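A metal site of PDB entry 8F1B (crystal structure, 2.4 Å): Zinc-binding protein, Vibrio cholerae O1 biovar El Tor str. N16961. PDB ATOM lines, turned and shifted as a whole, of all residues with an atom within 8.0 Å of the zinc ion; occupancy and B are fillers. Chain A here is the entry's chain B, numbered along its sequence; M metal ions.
ND1 of His 28 is bound to the zinc ion, 2.0 Å away. The side-chain carboxylate (OE2) of Glu 114 is bound to the zinc ion. NE2 of His 112 is bound to the zinc ion.
The backbone NH (N) of Cys 113 lies within hydrogen-bond range of the backbone carbonyl oxygen (O) of His 28. O of Gln 78 is in hydrogen-bond range of N of Glu 114 (3.0 Å). OD1 of Asp 29 is in hydrogen-bond range of ND1 of His 112 (2.9 Å). The backbone carbonyl oxygen (O) of His 112 lies within hydrogen-bond range of the backbone NH (N) of Glu 80.
Of the 11 residues printed, 3 come within 4 Å of the zinc ion. The nearest printed residue that does not touch the zinc ion is Cys 113 (5.1 Å).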
ATOM      1  N   GLY A  27      -0.319 -10.928  -1.870  1.00  0.00           N
ATOM      2  CA  GLY A  27       0.321 -10.112  -2.909  1.00  0.00           C
ATOM      3  C   GLY A  27       1.092 -11.000  -3.867  1.00  0.00           C
ATOM      4  O   GLY A  27       0.490 -11.952  -4.401  1.00  0.00           O
ATOM      5  N   HIS A  28       2.382 -10.749  -4.047  1.00  0.00           N
ATOM      6  CA  HIS A  28       3.223 -11.557  -4.973  1.00  0.00           C
ATOM      7  C   HIS A  28       3.770 -12.789  -4.250  1.00  0.00           C
ATOM      8  O   HIS A  28       4.354 -13.638  -4.940  1.00  0.00           O
ATOM      9  CB  HIS A  28       4.323 -10.700  -5.611  1.00  0.00           C
ATOM     10  CG  HIS A  28       3.805  -9.502  -6.337  1.00  0.00           C
ATOM     11  ND1 HIS A  28       4.628  -8.458  -6.744  1.00  0.00           N
ATOM     12  CD2 HIS A  28       2.550  -9.146  -6.680  1.00  0.00           C
ATOM     13  CE1 HIS A  28       3.907  -7.535  -7.331  1.00  0.00           C
ATOM     14  NE2 HIS A  28       2.626  -7.913  -7.289  1.00  0.00           N
ATOM     15  N   ASP A  29       3.587 -12.899  -2.935  1.00  0.00           N
ATOM     16  CA  ASP A  29       4.188 -13.997  -2.137  1.00  0.00           C
ATOM     17  C   ASP A  29       3.234 -15.187  -2.068  1.00  0.00           C
ATOM     18  O   ASP A  29       2.100 -15.017  -1.591  1.00  0.00           O
ATOM     19  CB  ASP A  29       4.591 -13.499  -0.748  1.00  0.00           C
ATOM     20  CG  ASP A  29       5.714 -12.480  -0.801  1.00  0.00           C
ATOM     21  OD1 ASP A  29       6.623 -12.640  -1.648  1.00  0.00           O
ATOM     22  OD2 ASP A  29       5.644 -11.510  -0.010  1.00  0.00           O
ATOM     23  N   GLN A  78       4.740 -16.296 -13.344  1.00  0.00           N
ATOM     24  CA  GLN A  78       6.113 -15.763 -13.171  1.00  0.00           C
ATOM     25  C   GLN A  78       6.550 -15.887 -11.703  1.00  0.00           C
ATOM     26  O   GLN A  78       6.822 -14.863 -11.063  1.00  0.00           O
ATOM     27  CB  GLN A  78       6.191 -14.292 -13.567  1.00  0.00           C
ATOM     28  CG  GLN A  78       5.615 -14.009 -14.950  1.00  0.00           C
ATOM     29  CD  GLN A  78       6.042 -12.646 -15.441  1.00  0.00           C
ATOM     30  OE1 GLN A  78       7.124 -12.160 -15.130  1.00  0.00           O
ATOM     31  NE2 GLN A  78       5.182 -12.000 -16.212  1.00  0.00           N
ATOM     32  N   GLU A  80       8.984 -17.054  -8.635  1.00  0.00           N
ATOM     33  CA  GLU A  80      10.419 -17.237  -8.335  1.00  0.00           C
ATOM     34  C   GLU A  80      10.549 -17.920  -6.972  1.00  0.00           C
ATOM     35  O   GLU A  80      10.004 -17.395  -5.996  1.00  0.00           O
ATOM     36  CB  GLU A  80      11.134 -15.891  -8.315  1.00  0.00           C
ATOM     37  CG  GLU A  80      11.176 -15.214  -9.672  1.00  0.00           C
ATOM     38  CD  GLU A  80      10.966 -13.699  -9.605  1.00  0.00           C
ATOM     39  OE1 GLU A  80      11.935 -12.974  -9.232  1.00  0.00           O
ATOM     40  OE2 GLU A  80       9.814 -13.259  -9.935  1.00  0.00           O
ATOM     41  N   ARG A  82      12.102 -18.352  -3.673  1.00  0.00           N
ATOM     42  CA  ARG A  82      12.796 -17.370  -2.815  1.00  0.00           C
ATOM     43  C   ARG A  82      13.178 -17.994  -1.481  1.00  0.00           C
ATOM     44  O   ARG A  82      14.107 -17.489  -0.862  1.00  0.00           O
ATOM     45  CB  ARG A  82      11.917 -16.147  -2.592  1.00  0.00           C
ATOM     46  CG  ARG A  82      11.833 -15.248  -3.812  1.00  0.00           C
ATOM     47  CD  ARG A  82      12.730 -14.031  -3.689  1.00  0.00           C
ATOM     48  NE  ARG A  82      12.210 -12.893  -4.444  1.00  0.00           N
ATOM     49  CZ  ARG A  82      12.245 -12.781  -5.762  1.00  0.00           C
ATOM     50  NH1 ARG A  82      12.780 -13.731  -6.513  1.00  0.00           N
ATOM     51  NH2 ARG A  82      11.734 -11.698  -6.327  1.00  0.00           N
ATOM     52  N   HIS A 112       7.784 -15.903  -5.095  1.00  0.00           N
ATOM     53  CA  HIS A 112       7.436 -14.500  -5.405  1.00  0.00           C
ATOM     54  C   HIS A 112       6.997 -14.480  -6.856  1.00  0.00           C
ATOM     55  O   HIS A 112       7.824 -14.763  -7.719  1.00  0.00           O
ATOM     56  CB  HIS A 112       8.615 -13.576  -5.129  1.00  0.00           C
ATOM     57  CG  HIS A 112       8.224 -12.147  -5.113  1.00  0.00           C
ATOM     58  ND1 HIS A 112       7.932 -11.474  -3.925  1.00  0.00           N
ATOM     59  CD2 HIS A 112       8.076 -11.251  -6.120  1.00  0.00           C
ATOM     60  CE1 HIS A 112       7.620 -10.226  -4.208  1.00  0.00           C
ATOM     61  NE2 HIS A 112       7.685 -10.065  -5.556  1.00  0.00           N
ATOM     62  N   CYS A 113       5.711 -14.254  -7.083  1.00  0.00           N
ATOM     63  CA  CYS A 113       5.095 -14.345  -8.425  1.00  0.00           C
ATOM     64  C   CYS A 113       4.748 -12.926  -8.877  1.00  0.00           C
ATOM     65  O   CYS A 113       3.859 -12.295  -8.236  1.00  0.00           O
ATOM     66  CB  CYS A 113       3.854 -15.228  -8.396  1.00  0.00           C
ATOM     67  SG  CYS A 113       4.121 -16.852  -7.655  1.00  0.00           S
ATOM     68  N   GLU A 114       5.409 -12.428  -9.910  1.00  0.00           N
ATOM     69  CA  GLU A 114       5.181 -11.045 -10.392  1.00  0.00           C
ATOM     70  C   GLU A 114       3.818 -10.923 -11.078  1.00  0.00           C
ATOM     71  O   GLU A 114       3.295  -9.802 -11.135  1.00  0.00           O
ATOM     72  CB  GLU A 114       6.313 -10.557 -11.296  1.00  0.00           C
ATOM     73  CG  GLU A 114       7.488  -9.999 -10.523  1.00  0.00           C
ATOM     74  CD  GLU A 114       7.112  -9.102  -9.347  1.00  0.00           C
ATOM     75  OE1 GLU A 114       6.442  -8.096  -9.583  1.00  0.00           O
ATOM     76  OE2 GLU A 114       7.489  -9.421  -8.204  1.00  0.00           O
ATOM     77  N   ALA A 115       3.266 -12.034 -11.568  1.00  0.00           N
ATOM     78  CA  ALA A 115       1.910 -12.072 -12.165  1.00  0.00           C
ATOM     79  C   ALA A 115       1.031 -13.042 -11.357  1.00  0.00           C
ATOM     80  O   ALA A 115       0.412 -13.943 -11.942  1.00  0.00           O
ATOM     81  CB  ALA A 115       2.006 -12.444 -13.608  1.00  0.00           C
ATOM     82  N   VAL A 116       0.982 -12.848 -10.041  1.00  0.00           N
ATOM     83  CA  VAL A 116       0.308 -13.796  -9.107  1.00  0.00           C
ATOM     84  C   VAL A 116      -1.160 -14.003  -9.514  1.00  0.00           C
ATOM     85  O   VAL A 116      -1.734 -15.026  -9.121  1.00  0.00           O
ATOM     86  CB  VAL A 116       0.431 -13.325  -7.641  1.00  0.00           C
ATOM     87  CG1 VAL A 116      -0.294 -12.007  -7.402  1.00  0.00           C
ATOM     88  CG2 VAL A 116      -0.068 -14.390  -6.688  1.00  0.00           C
HETATM   89 ZN    ZN M   1       6.631  -8.330  -6.689  1.00  0.00          ZN
